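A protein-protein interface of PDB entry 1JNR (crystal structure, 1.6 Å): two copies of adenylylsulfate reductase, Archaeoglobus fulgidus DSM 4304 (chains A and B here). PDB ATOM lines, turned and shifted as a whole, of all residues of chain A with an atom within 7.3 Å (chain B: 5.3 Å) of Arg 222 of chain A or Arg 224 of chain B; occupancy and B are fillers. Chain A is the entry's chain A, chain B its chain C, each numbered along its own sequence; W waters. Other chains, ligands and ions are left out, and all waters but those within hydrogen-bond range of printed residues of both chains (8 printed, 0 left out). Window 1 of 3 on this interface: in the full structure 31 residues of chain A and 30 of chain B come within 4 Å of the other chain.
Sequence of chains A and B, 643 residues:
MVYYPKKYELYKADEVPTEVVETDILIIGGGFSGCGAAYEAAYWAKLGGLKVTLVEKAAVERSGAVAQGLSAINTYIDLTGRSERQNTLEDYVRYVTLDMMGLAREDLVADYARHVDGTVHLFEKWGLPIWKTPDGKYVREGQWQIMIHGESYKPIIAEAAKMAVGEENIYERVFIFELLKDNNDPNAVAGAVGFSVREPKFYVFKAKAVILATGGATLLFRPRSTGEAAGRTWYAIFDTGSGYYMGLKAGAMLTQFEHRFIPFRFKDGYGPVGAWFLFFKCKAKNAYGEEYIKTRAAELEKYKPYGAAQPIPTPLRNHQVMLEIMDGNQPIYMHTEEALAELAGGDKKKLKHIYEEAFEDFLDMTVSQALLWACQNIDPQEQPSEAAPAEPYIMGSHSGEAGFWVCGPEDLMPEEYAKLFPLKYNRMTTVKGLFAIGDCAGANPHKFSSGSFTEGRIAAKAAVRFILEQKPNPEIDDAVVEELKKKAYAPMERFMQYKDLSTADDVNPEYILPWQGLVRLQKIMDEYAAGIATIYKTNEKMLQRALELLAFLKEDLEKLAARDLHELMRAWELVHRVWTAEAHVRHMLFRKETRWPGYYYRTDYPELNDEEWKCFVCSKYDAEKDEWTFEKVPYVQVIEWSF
Among the printed residues, pairs that only touch across the chains: Arg 222 of chain A with Ser 225 of chain B (3.9 Å), Arg 222 of chain A with Thr 226 of chain B (3.9 Å), Ser 225 of chain A with Arg 222 of chain B (3.8 Å), Thr 226 of chain A with Arg 222 of chain B (3.7 Å) and Thr 226 of chain A with Thr 226 of chain B (3.5 Å).
NE of Arg 222 of chain A is in salt-bridge range of OD2 of Asp 526 of chain A (2.6 Å).
The guanidinium group (NH2) of Arg 222 of chain A lies within salt-bridge range of the side-chain carboxylate (OE2) of Glu 527 of chain A (3.3 Å).
NH2 of Arg 224 of chain B sits at hydrogen-bond distance from OH of Tyr 536 of chain B (3.0 Å).
Water W7 bridges the backbone carbonyl oxygen of Thr 226 of chain A and the backbone carbonyl oxygen of Thr 226 of chain B.
Arg 222 of chain A touches Arg 224 of chain B, and with the chains exchanged Arg 224 of chain A touches Arg 222 of chain B.
Arg 222 of chain A touches Ser 225 of chain B, and with the chains exchanged Ser 225 of chain A touches Arg 222 of chain B.
Thr 226 of chain A touches its own counterpart, Thr 226 of chain B.
Arg 222 of chain A touches just these residues of chain B: Arg 224 (2.9 Å), Ser 225 (3.9 Å) and Thr 226 (3.9 Å).
Of the printed residues of chain A, Arg 224 of chain B touches Arg 222 (2.9 Å), Lys 523 (3.0 Å) and Glu 527 (3.5 Å).
Printed residues of chain B within 4 Å of Ser 225 of chain A: Arg 222.
Of the printed residues of chain A, Thr 226 of chain B touches Arg 222 (3.9 Å) and Thr 226 (3.5 Å).
The nearest residue of chain A that does not touch Arg 224 of chain B is Ala 533 of chain A (5.2 Å).
The nearest printed residue of chain B that does not touch Ser 225 of chain A is Thr 226 of chain B (6.9 Å).
Printed residues of chain B that touch a printed residue of chain A: Arg 222, Arg 224, Ser 225 and Thr 226.
Among the printed residues, 10 pairs touch across the chains.
Among the printed residues, no Asp or Glu carboxylate lies within 4 Å of a Lys or Arg side-chain nitrogen of the other chain.
O of Arg 224 of chain B is in hydrogen-bond range of NH1 of Arg 222 of chain A, at 2.9 Å.
The guanidinium group (NH1) of Arg 222 of chain B lies within hydrogen-bond range of the backbone carbonyl oxygen (O) of Arg 224 of chain A, at 2.8 Å.
The backbone carbonyl oxygen (O) of Arg 224 of chain B is in hydrogen-bond range of the side-chain amino group (NZ) of Lys 523 of chain A (3.0 Å).
The side-chain hydroxyl of Ser 225 of chain B lies within hydrogen-bond range of the side-chain amino group of Lys 523 of chain A, at 3.0 Å.
The side-chain carboxylate (OE2) of Glu 527 of chain A sits close to the backbone carbonyl oxygen (O) of Arg 224 of chain B, 3.5 Å away.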
ATOM      1  N   LEU A 219       6.490 -18.292  16.616  1.00  0.00           N
ATOM      2  CA  LEU A 219       6.576 -18.007  15.188  1.00  0.00           C
ATOM      3  C   LEU A 219       7.694 -17.035  14.812  1.00  0.00           C
ATOM      4  O   LEU A 219       7.648 -16.394  13.761  1.00  0.00           O
ATOM      5  CB  LEU A 219       5.226 -17.535  14.627  1.00  0.00           C
ATOM      6  CG  LEU A 219       4.181 -18.655  14.479  1.00  0.00           C
ATOM      7  CD1 LEU A 219       2.956 -18.107  13.762  1.00  0.00           C
ATOM      8  CD2 LEU A 219       4.758 -19.825  13.686  1.00  0.00           C
ATOM      9  N   LEU A 220       8.694 -16.927  15.686  1.00  0.00           N
ATOM     10  CA  LEU A 220       9.866 -16.103  15.405  1.00  0.00           C
ATOM     11  C   LEU A 220      10.746 -16.973  14.515  1.00  0.00           C
ATOM     12  O   LEU A 220      11.400 -16.488  13.590  1.00  0.00           O
ATOM     13  CB  LEU A 220      10.646 -15.784  16.681  1.00  0.00           C
ATOM     14  CG  LEU A 220      10.408 -14.423  17.330  1.00  0.00           C
ATOM     15  CD1 LEU A 220       9.008 -14.368  17.904  1.00  0.00           C
ATOM     16  CD2 LEU A 220      11.450 -14.186  18.412  1.00  0.00           C
ATOM     17  N   PHE A 221      10.750 -18.270  14.818  1.00  0.00           N
ATOM     18  CA  PHE A 221      11.539 -19.250  14.078  1.00  0.00           C
ATOM     19  C   PHE A 221      10.694 -20.097  13.135  1.00  0.00           C
ATOM     20  O   PHE A 221       9.550 -20.431  13.437  1.00  0.00           O
ATOM     21  CB  PHE A 221      12.260 -20.210  15.033  1.00  0.00           C
ATOM     22  CG  PHE A 221      13.403 -19.593  15.790  1.00  0.00           C
ATOM     23  CD1 PHE A 221      13.177 -18.815  16.923  1.00  0.00           C
ATOM     24  CD2 PHE A 221      14.716 -19.808  15.376  1.00  0.00           C
ATOM     25  CE1 PHE A 221      14.246 -18.265  17.634  1.00  0.00           C
ATOM     26  CE2 PHE A 221      15.787 -19.263  16.077  1.00  0.00           C
ATOM     27  CZ  PHE A 221      15.556 -18.493  17.205  1.00  0.00           C
ATOM     28  N   ARG A 222      11.274 -20.450  11.996  1.00  0.00           N
ATOM     29  CA  ARG A 222      10.592 -21.301  11.030  1.00  0.00           C
ATOM     30  C   ARG A 222      10.272 -22.643  11.702  1.00  0.00           C
ATOM     31  O   ARG A 222      11.142 -23.263  12.311  1.00  0.00           O
ATOM     32  CB  ARG A 222      11.495 -21.522   9.807  1.00  0.00           C
ATOM     33  CG  ARG A 222      11.033 -22.646   8.897  1.00  0.00           C
ATOM     34  CD  ARG A 222      11.588 -22.505   7.484  1.00  0.00           C
ATOM     35  NE  ARG A 222      13.026 -22.308   7.419  1.00  0.00           N
ATOM     36  CZ  ARG A 222      13.653 -21.847   6.344  1.00  0.00           C
ATOM     37  NH1 ARG A 222      12.955 -21.535   5.263  1.00  0.00           N
ATOM     38  NH2 ARG A 222      14.972 -21.704   6.342  1.00  0.00           N
ATOM     39  N   PRO A 223       9.014 -23.103  11.617  1.00  0.00           N
ATOM     40  CA  PRO A 223       8.655 -24.384  12.241  1.00  0.00           C
ATOM     41  C   PRO A 223       9.058 -25.584  11.385  1.00  0.00           C
ATOM     42  O   PRO A 223       9.560 -25.425  10.270  1.00  0.00           O
ATOM     43  CB  PRO A 223       7.131 -24.293  12.390  1.00  0.00           C
ATOM     44  CG  PRO A 223       6.843 -22.815  12.315  1.00  0.00           C
ATOM     45  CD  PRO A 223       7.804 -22.348  11.256  1.00  0.00           C
ATOM     46  N   ARG A 224       8.831 -26.782  11.914  1.00  0.00           N
ATOM     47  CA  ARG A 224       9.158 -28.004  11.189  1.00  0.00           C
ATOM     48  C   ARG A 224       8.107 -28.333  10.136  1.00  0.00           C
ATOM     49  O   ARG A 224       8.259 -29.277   9.361  1.00  0.00           O
ATOM     50  CB  ARG A 224       9.334 -29.171  12.160  1.00  0.00           C
ATOM     51  CG  ARG A 224      10.598 -29.031  13.006  1.00  0.00           C
ATOM     52  CD  ARG A 224      10.990 -30.330  13.667  1.00  0.00           C
ATOM     53  NE  ARG A 224      12.226 -30.192  14.436  1.00  0.00           N
ATOM     54  CZ  ARG A 224      13.451 -30.198  13.914  1.00  0.00           C
ATOM     55  NH1 ARG A 224      13.630 -30.340  12.606  1.00  0.00           N
ATOM     56  NH2 ARG A 224      14.505 -30.055  14.704  1.00  0.00           N
ATOM     57  N   SER A 225       7.034 -27.553  10.131  1.00  0.00           N
ATOM     58  CA  SER A 225       5.963 -27.692   9.152  1.00  0.00           C
ATOM     59  C   SER A 225       5.725 -26.262   8.688  1.00  0.00           C
ATOM     60  O   SER A 225       5.489 -25.369   9.503  1.00  0.00           O
ATOM     61  CB  SER A 225       4.705 -28.284   9.785  1.00  0.00           C
ATOM     62  OG  SER A 225       4.885 -29.664  10.067  1.00  0.00           O
ATOM     63  N   THR A 226       5.792 -26.050   7.379  1.00  0.00           N
ATOM     64  CA  THR A 226       5.671 -24.710   6.825  1.00  0.00           C
ATOM     65  C   THR A 226       4.431 -24.401   6.004  1.00  0.00           C
ATOM     66  O   THR A 226       4.320 -23.309   5.444  1.00  0.00           O
ATOM     67  CB  THR A 226       6.913 -24.391   5.980  1.00  0.00           C
ATOM     68  OG1 THR A 226       7.111 -25.437   5.023  1.00  0.00           O
ATOM     69  CG2 THR A 226       8.147 -24.300   6.869  1.00  0.00           C
ATOM     70  N   ALA A 390      10.952 -29.366  18.700  1.00  0.00           N
ATOM     71  CA  ALA A 390      10.367 -28.358  17.822  1.00  0.00           C
ATOM     72  C   ALA A 390      11.329 -27.188  17.657  1.00  0.00           C
ATOM     73  O   ALA A 390      12.442 -27.212  18.184  1.00  0.00           O
ATOM     74  CB  ALA A 390       9.045 -27.867  18.399  1.00  0.00           C
ATOM     75  N   GLU A 391      10.905 -26.166  16.918  1.00  0.00           N
ATOM     76  CA  GLU A 391      11.748 -24.990  16.737  1.00  0.00           C
ATOM     77  C   GLU A 391      11.731 -24.200  18.053  1.00  0.00           C
ATOM     78  O   GLU A 391      10.901 -24.453  18.930  1.00  0.00           O
ATOM     79  CB  GLU A 391      11.248 -24.127  15.565  1.00  0.00           C
ATOM     80  CG  GLU A 391       9.989 -23.314  15.832  1.00  0.00           C
ATOM     81  CD  GLU A 391       8.704 -24.127  15.769  1.00  0.00           C
ATOM     82  OE1 GLU A 391       8.771 -25.370  15.658  1.00  0.00           O
ATOM     83  OE2 GLU A 391       7.621 -23.509  15.835  1.00  0.00           O
ATOM     84  N   PRO A 392      12.648 -23.236  18.215  1.00  0.00           N
ATOM     85  CA  PRO A 392      12.708 -22.442  19.452  1.00  0.00           C
ATOM     86  C   PRO A 392      11.547 -21.495  19.731  1.00  0.00           C
ATOM     87  O   PRO A 392      10.942 -20.939  18.812  1.00  0.00           O
ATOM     88  CB  PRO A 392      14.015 -21.657  19.310  1.00  0.00           C
ATOM     89  CG  PRO A 392      14.808 -22.443  18.301  1.00  0.00           C
ATOM     90  CD  PRO A 392      13.769 -22.904  17.324  1.00  0.00           C
ATOM     91  N   LEU A 518       6.726 -12.066   7.961  1.00  0.00           N
ATOM     92  CA  LEU A 518       6.882 -13.155   8.922  1.00  0.00           C
ATOM     93  C   LEU A 518       7.696 -14.305   8.330  1.00  0.00           C
ATOM     94  O   LEU A 518       8.538 -14.891   9.013  1.00  0.00           O
ATOM     95  CB  LEU A 518       5.513 -13.663   9.391  1.00  0.00           C
ATOM     96  CG  LEU A 518       5.559 -14.660  10.553  1.00  0.00           C
ATOM     97  CD1 LEU A 518       6.376 -14.076  11.702  1.00  0.00           C
ATOM     98  CD2 LEU A 518       4.143 -14.975  11.012  1.00  0.00           C
ATOM     99  N   VAL A 519       7.441 -14.633   7.066  1.00  0.00           N
ATOM    100  CA  VAL A 519       8.196 -15.688   6.396  1.00  0.00           C
ATOM    101  C   VAL A 519       9.669 -15.290   6.413  1.00  0.00           C
ATOM    102  O   VAL A 519      10.548 -16.106   6.673  1.00  0.00           O
ATOM    103  CB  VAL A 519       7.741 -15.856   4.924  1.00  0.00           C
ATOM    104  CG1 VAL A 519       8.775 -16.662   4.138  1.00  0.00           C
ATOM    105  CG2 VAL A 519       6.400 -16.556   4.879  1.00  0.00           C
ATOM    106  N   LEU A 521      11.214 -13.190   8.529  1.00  0.00           N
ATOM    107  CA  LEU A 521      11.731 -13.257   9.890  1.00  0.00           C
ATOM    108  C   LEU A 521      12.089 -14.694  10.246  1.00  0.00           C
ATOM    109  O   LEU A 521      13.183 -14.969  10.733  1.00  0.00           O
ATOM    110  CB  LEU A 521      10.691 -12.742  10.888  1.00  0.00           C
ATOM    111  CG  LEU A 521      11.101 -12.905  12.357  1.00  0.00           C
ATOM    112  CD1 LEU A 521      12.370 -12.095  12.611  1.00  0.00           C
ATOM    113  CD2 LEU A 521       9.977 -12.448  13.275  1.00  0.00           C
ATOM    114  N   GLN A 522      11.161 -15.610   9.996  1.00  0.00           N
ATOM    115  CA  GLN A 522      11.378 -17.016  10.317  1.00  0.00           C
ATOM    116  C   GLN A 522      12.580 -17.637   9.624  1.00  0.00           C
ATOM    117  O   GLN A 522      13.262 -18.483  10.211  1.00  0.00           O
ATOM    118  CB  GLN A 522      10.118 -17.824  10.000  1.00  0.00           C
ATOM    119  CG  GLN A 522       8.967 -17.497  10.938  1.00  0.00           C
ATOM    120  CD  GLN A 522       7.677 -18.179  10.547  1.00  0.00           C
ATOM    121  OE1 GLN A 522       7.626 -18.930   9.572  1.00  0.00           O
ATOM    122  NE2 GLN A 522       6.618 -17.918  11.308  1.00  0.00           N
ATOM    123  N   LYS A 523      12.841 -17.228   8.384  1.00  0.00           N
ATOM    124  CA  LYS A 523      13.974 -17.763   7.636  1.00  0.00           C
ATOM    125  C   LYS A 523      15.283 -17.237   8.230  1.00  0.00           C
ATOM    126  O   LYS A 523      16.240 -17.986   8.406  1.00  0.00           O
ATOM    127  CB  LYS A 523      13.857 -17.380   6.153  1.00  0.00           C
ATOM    128  CG  LYS A 523      15.005 -17.874   5.272  1.00  0.00           C
ATOM    129  CD  LYS A 523      14.744 -17.530   3.803  1.00  0.00           C
ATOM    130  CE  LYS A 523      15.982 -17.735   2.926  1.00  0.00           C
ATOM    131  NZ  LYS A 523      16.427 -19.154   2.845  1.00  0.00           N
ATOM    132  N   ILE A 524      15.321 -15.943   8.536  1.00  0.00           N
ATOM    133  CA  ILE A 524      16.510 -15.343   9.126  1.00  0.00           C
ATOM    134  C   ILE A 524      16.858 -16.017  10.449  1.00  0.00           C
ATOM    135  O   ILE A 524      17.997 -16.422  10.678  1.00  0.00           O
ATOM    136  CB  ILE A 524      16.298 -13.845   9.414  1.00  0.00           C
ATOM    137  CG1 ILE A 524      16.139 -13.079   8.101  1.00  0.00           C
ATOM    138  CG2 ILE A 524      17.474 -13.296  10.211  1.00  0.00           C
ATOM    139  CD1 ILE A 524      15.701 -11.643   8.295  1.00  0.00           C
ATOM    140  N   MET A 525      15.874 -16.126  11.330  1.00  0.00           N
ATOM    141  CA  MET A 525      16.108 -16.732  12.632  1.00  0.00           C
ATOM    142  C   MET A 525      16.460 -18.212  12.526  1.00  0.00           C
ATOM    143  O   MET A 525      17.348 -18.701  13.221  1.00  0.00           O
ATOM    144  CB  MET A 525      14.882 -16.528  13.521  1.00  0.00           C
ATOM    145  CG  MET A 525      14.576 -15.061  13.786  1.00  0.00           C
ATOM    146  SD  MET A 525      15.930 -14.225  14.650  1.00  0.00           S
ATOM    147  CE  MET A 525      15.667 -14.837  16.316  1.00  0.00           C
ATOM    148  N   ASP A 526      15.777 -18.920  11.638  1.00  0.00           N
ATOM    149  CA  ASP A 526      16.037 -20.336  11.453  1.00  0.00           C
ATOM    150  C   ASP A 526      17.468 -20.605  10.990  1.00  0.00           C
ATOM    151  O   ASP A 526      18.151 -21.483  11.518  1.00  0.00           O
ATOM    152  CB  ASP A 526      15.046 -20.902  10.435  1.00  0.00           C
ATOM    153  CG  ASP A 526      15.231 -22.385  10.199  1.00  0.00           C
ATOM    154  OD1 ASP A 526      15.543 -23.105  11.169  1.00  0.00           O
ATOM    155  OD2 ASP A 526      15.051 -22.822   9.044  1.00  0.00           O
ATOM    156  N   GLU A 527      17.930 -19.823  10.025  1.00  0.00           N
ATOM    157  CA  GLU A 527      19.256 -20.025   9.457  1.00  0.00           C
ATOM    158  C   GLU A 527      20.434 -19.421  10.213  1.00  0.00           C
ATOM    159  O   GLU A 527      21.548 -19.932  10.124  1.00  0.00           O
ATOM    160  CB  GLU A 527      19.260 -19.521   8.013  1.00  0.00           C
ATOM    161  CG  GLU A 527      18.160 -20.158   7.178  1.00  0.00           C
ATOM    162  CD  GLU A 527      18.145 -19.684   5.744  1.00  0.00           C
ATOM    163  OE1 GLU A 527      18.564 -18.539   5.487  1.00  0.00           O
ATOM    164  OE2 GLU A 527      17.690 -20.458   4.880  1.00  0.00           O
ATOM    165  N   GLY A 531      18.294 -22.059  14.819  1.00  0.00           N
ATOM    166  CA  GLY A 531      16.984 -22.640  14.587  1.00  0.00           C
ATOM    167  C   GLY A 531      17.158 -24.100  14.203  1.00  0.00           C
ATOM    168  O   GLY A 531      18.263 -24.645  14.279  1.00  0.00           O
ATOM    169  N   ILE A 532      16.076 -24.741  13.777  1.00  0.00           N
ATOM    170  CA  ILE A 532      16.141 -26.148  13.399  1.00  0.00           C
ATOM    171  C   ILE A 532      17.048 -26.394  12.196  1.00  0.00           C
ATOM    172  O   ILE A 532      17.607 -27.483  12.049  1.00  0.00           O
ATOM    173  CB  ILE A 532      14.735 -26.700  13.084  1.00  0.00           C
ATOM    174  CG1 ILE A 532      14.128 -25.949  11.896  1.00  0.00           C
ATOM    175  CG2 ILE A 532      13.843 -26.573  14.315  1.00  0.00           C
ATOM    176  CD1 ILE A 532      12.740 -26.441  11.506  1.00  0.00           C
ATOM    177  N   ALA A 533      17.206 -25.381  11.346  1.00  0.00           N
ATOM    178  CA  ALA A 533      18.028 -25.502  10.144  1.00  0.00           C
ATOM    179  C   ALA A 533      19.457 -25.953  10.421  1.00  0.00           C
ATOM    180  O   ALA A 533      20.052 -26.665   9.613  1.00  0.00           O
ATOM    181  CB  ALA A 533      18.049 -24.174   9.393  1.00  0.00           C
ATOM    182  N   THR A 534      20.005 -25.528  11.553  1.00  0.00           N
ATOM    183  CA  THR A 534      21.374 -25.887  11.911  1.00  0.00           C
ATOM    184  C   THR A 534      21.445 -26.724  13.183  1.00  0.00           C
ATOM    185  O   THR A 534      22.464 -26.739  13.872  1.00  0.00           O
ATOM    186  CB  THR A 534      22.229 -24.624  12.110  1.00  0.00           C
ATOM    187  OG1 THR A 534      21.665 -23.828  13.160  1.00  0.00           O
ATOM    188  CG2 THR A 534      22.277 -23.805  10.826  1.00  0.00           C
ATOM    189  N   ARG B 222      11.524 -30.326   0.381  1.00  0.00           N
ATOM    190  CA  ARG B 222      11.265 -28.991   0.897  1.00  0.00           C
ATOM    191  C   ARG B 222      12.509 -28.127   0.649  1.00  0.00           C
ATOM    192  O   ARG B 222      13.629 -28.527   0.962  1.00  0.00           O
ATOM    193  CB  ARG B 222      10.957 -29.057   2.395  1.00  0.00           C
ATOM    194  CG  ARG B 222      10.754 -27.701   3.050  1.00  0.00           C
ATOM    195  CD  ARG B 222       9.894 -27.832   4.294  1.00  0.00           C
ATOM    196  NE  ARG B 222      10.427 -28.826   5.219  1.00  0.00           N
ATOM    197  CZ  ARG B 222       9.774 -29.280   6.284  1.00  0.00           C
ATOM    198  NH1 ARG B 222       8.558 -28.833   6.562  1.00  0.00           N
ATOM    199  NH2 ARG B 222      10.339 -30.183   7.072  1.00  0.00           N
ATOM    200  N   PRO B 223      12.329 -26.934   0.067  1.00  0.00           N
ATOM    201  CA  PRO B 223      13.462 -26.040  -0.206  1.00  0.00           C
ATOM    202  C   PRO B 223      13.916 -25.283   1.043  1.00  0.00           C
ATOM    203  O   PRO B 223      13.270 -25.356   2.093  1.00  0.00           O
ATOM    204  CB  PRO B 223      12.906 -25.082  -1.265  1.00  0.00           C
ATOM    205  CG  PRO B 223      11.742 -25.837  -1.865  1.00  0.00           C
ATOM    206  CD  PRO B 223      11.131 -26.486  -0.659  1.00  0.00           C
ATOM    207  N   ARG B 224      15.015 -24.541   0.920  1.00  0.00           N
ATOM    208  CA  ARG B 224      15.535 -23.756   2.040  1.00  0.00           C
ATOM    209  C   ARG B 224      14.731 -22.479   2.243  1.00  0.00           C
ATOM    210  O   ARG B 224      14.952 -21.732   3.192  1.00  0.00           O
ATOM    211  CB  ARG B 224      17.008 -23.423   1.828  1.00  0.00           C
ATOM    212  CG  ARG B 224      17.903 -24.642   1.942  1.00  0.00           C
ATOM    213  CD  ARG B 224      19.360 -24.270   2.068  1.00  0.00           C
ATOM    214  NE  ARG B 224      20.188 -25.459   2.256  1.00  0.00           N
ATOM    215  CZ  ARG B 224      20.281 -26.149   3.391  1.00  0.00           C
ATOM    216  NH1 ARG B 224      19.597 -25.774   4.466  1.00  0.00           N
ATOM    217  NH2 ARG B 224      21.059 -27.223   3.449  1.00  0.00           N
ATOM    218  N   SER B 225      13.809 -22.231   1.323  1.00  0.00           N
ATOM    219  CA  SER B 225      12.910 -21.088   1.405  1.00  0.00           C
ATOM    220  C   SER B 225      11.548 -21.718   1.169  1.00  0.00           C
ATOM    221  O   SER B 225      11.350 -22.438   0.187  1.00  0.00           O
ATOM    222  CB  SER B 225      13.241 -20.045   0.335  1.00  0.00           C
ATOM    223  OG  SER B 225      14.457 -19.387   0.645  1.00  0.00           O
ATOM    224  N   THR B 226      10.613 -21.464   2.076  1.00  0.00           N
ATOM    225  CA  THR B 226       9.297 -22.082   1.982  1.00  0.00           C
ATOM    226  C   THR B 226       8.110 -21.167   1.725  1.00  0.00           C
ATOM    227  O   THR B 226       6.967 -21.620   1.762  1.00  0.00           O
ATOM    228  CB  THR B 226       9.011 -22.891   3.246  1.00  0.00           C
ATOM    229  OG1 THR B 226       9.165 -22.041   4.383  1.00  0.00           O
ATOM    230  CG2 THR B 226       9.984 -24.059   3.370  1.00  0.00           C
ATOM    231  N   TYR B 270      20.730 -18.917  -5.540  1.00  0.00           N
ATOM    232  CA  TYR B 270      21.346 -20.032  -6.249  1.00  0.00           C
ATOM    233  C   TYR B 270      22.025 -19.670  -7.557  1.00  0.00           C
ATOM    234  O   TYR B 270      22.010 -20.443  -8.520  1.00  0.00           O
ATOM    235  CB  TYR B 270      20.319 -21.148  -6.448  1.00  0.00           C
ATOM    236  CG  TYR B 270      19.849 -21.709  -5.124  1.00  0.00           C
ATOM    237  CD1 TYR B 270      18.499 -21.938  -4.879  1.00  0.00           C
ATOM    238  CD2 TYR B 270      20.763 -21.989  -4.101  1.00  0.00           C
ATOM    239  CE1 TYR B 270      18.064 -22.429  -3.649  1.00  0.00           C
ATOM    240  CE2 TYR B 270      20.338 -22.479  -2.871  1.00  0.00           C
ATOM    241  CZ  TYR B 270      18.988 -22.696  -2.653  1.00  0.00           C
ATOM    242  OH  TYR B 270      18.560 -23.172  -1.435  1.00  0.00           O
ATOM    243  N   ALA B 388      25.650 -21.802  -0.292  1.00  0.00           N
ATOM    244  CA  ALA B 388      25.055 -22.909   0.437  1.00  0.00           C
ATOM    245  C   ALA B 388      24.541 -23.988  -0.498  1.00  0.00           C
ATOM    246  O   ALA B 388      24.259 -23.730  -1.672  1.00  0.00           O
ATOM    247  CB  ALA B 388      23.907 -22.395   1.304  1.00  0.00           C
ATOM    248  N   PRO B 389      24.439 -25.227   0.007  1.00  0.00           N
ATOM    249  CA  PRO B 389      23.936 -26.329  -0.812  1.00  0.00           C
ATOM    250  C   PRO B 389      22.408 -26.278  -0.750  1.00  0.00           C
ATOM    251  O   PRO B 389      21.839 -26.071   0.322  1.00  0.00           O
ATOM    252  CB  PRO B 389      24.506 -27.562  -0.119  1.00  0.00           C
ATOM    253  CG  PRO B 389      24.528 -27.157   1.324  1.00  0.00           C
ATOM    254  CD  PRO B 389      25.021 -25.720   1.271  1.00  0.00           C
ATOM    255  N   ALA B 390      21.751 -26.439  -1.892  1.00  0.00           N
ATOM    256  CA  ALA B 390      20.292 -26.415  -1.931  1.00  0.00           C
ATOM    257  C   ALA B 390      19.750 -27.795  -1.576  1.00  0.00           C
ATOM    258  O   ALA B 390      20.516 -28.705  -1.254  1.00  0.00           O
ATOM    259  CB  ALA B 390      19.807 -26.007  -3.321  1.00  0.00           C
ATOM    260  N   GLU B 391      18.430 -27.946  -1.621  1.00  0.00           N
ATOM    261  CA  GLU B 391      17.819 -29.236  -1.331  1.00  0.00           C
ATOM    262  C   GLU B 391      18.086 -30.130  -2.548  1.00  0.00           C
ATOM    263  O   GLU B 391      18.509 -29.644  -3.597  1.00  0.00           O
ATOM    264  CB  GLU B 391      16.312 -29.076  -1.081  1.00  0.00           C
ATOM    265  CG  GLU B 391      15.466 -28.824  -2.324  1.00  0.00           C
ATOM    266  CD  GLU B 391      15.476 -27.377  -2.802  1.00  0.00           C
ATOM    267  OE1 GLU B 391      16.278 -26.560  -2.298  1.00  0.00           O
ATOM    268  OE2 GLU B 391      14.665 -27.064  -3.696  1.00  0.00           O
ATOM    269  N   ILE B 532      17.405 -31.458   3.409  1.00  0.00           N
ATOM    270  CA  ILE B 532      18.167 -30.466   4.162  1.00  0.00           C
ATOM    271  C   ILE B 532      17.948 -30.554   5.673  1.00  0.00           C
ATOM    272  O   ILE B 532      18.826 -30.172   6.449  1.00  0.00           O
ATOM    273  CB  ILE B 532      17.829 -29.026   3.705  1.00  0.00           C
ATOM    274  CG1 ILE B 532      16.362 -28.702   4.006  1.00  0.00           C
ATOM    275  CG2 ILE B 532      18.100 -28.879   2.218  1.00  0.00           C
ATOM    276  CD1 ILE B 532      15.963 -27.289   3.630  1.00  0.00           C
ATOM    277  N   TYR B 536      21.259 -33.917   4.740  1.00  0.00           N
ATOM    278  CA  TYR B 536      21.349 -34.990   3.753  1.00  0.00           C
ATOM    279  C   TYR B 536      21.668 -36.393   4.283  1.00  0.00           C
ATOM    280  O   TYR B 536      22.216 -37.226   3.557  1.00  0.00           O
ATOM    281  CB  TYR B 536      22.359 -34.587   2.672  1.00  0.00           C
ATOM    282  CG  TYR B 536      22.195 -33.146   2.227  1.00  0.00           C
ATOM    283  CD1 TYR B 536      22.999 -32.137   2.756  1.00  0.00           C
ATOM    284  CD2 TYR B 536      21.191 -32.784   1.330  1.00  0.00           C
ATOM    285  CE1 TYR B 536      22.804 -30.800   2.406  1.00  0.00           C
ATOM    286  CE2 TYR B 536      20.991 -31.450   0.974  1.00  0.00           C
ATOM    287  CZ  TYR B 536      21.797 -30.468   1.516  1.00  0.00           C
ATOM    288  OH  TYR B 536      21.596 -29.149   1.179  1.00  0.00           O
HETATM  289  O   HOH W   1       5.603 -28.590   6.053  1.00  0.00           O
HETATM  290  O   HOH W   2      18.119 -23.258   5.162  1.00  0.00           O
HETATM  291  O   HOH W   3       6.298 -24.337   2.677  1.00  0.00           O
HETATM  292  O   HOH W   4      11.370 -19.263   3.692  1.00  0.00           O
HETATM  293  O   HOH W   5      10.088 -26.950   8.234  1.00  0.00           O
HETATM  294  O   HOH W   6      19.094 -27.118   7.057  1.00  0.00           O
HETATM  295  O   HOH W   7       5.763 -21.163   4.423  1.00  0.00           O
HETATM  296  O   HOH W   8      13.440 -24.315   4.493  1.00  0.00           O
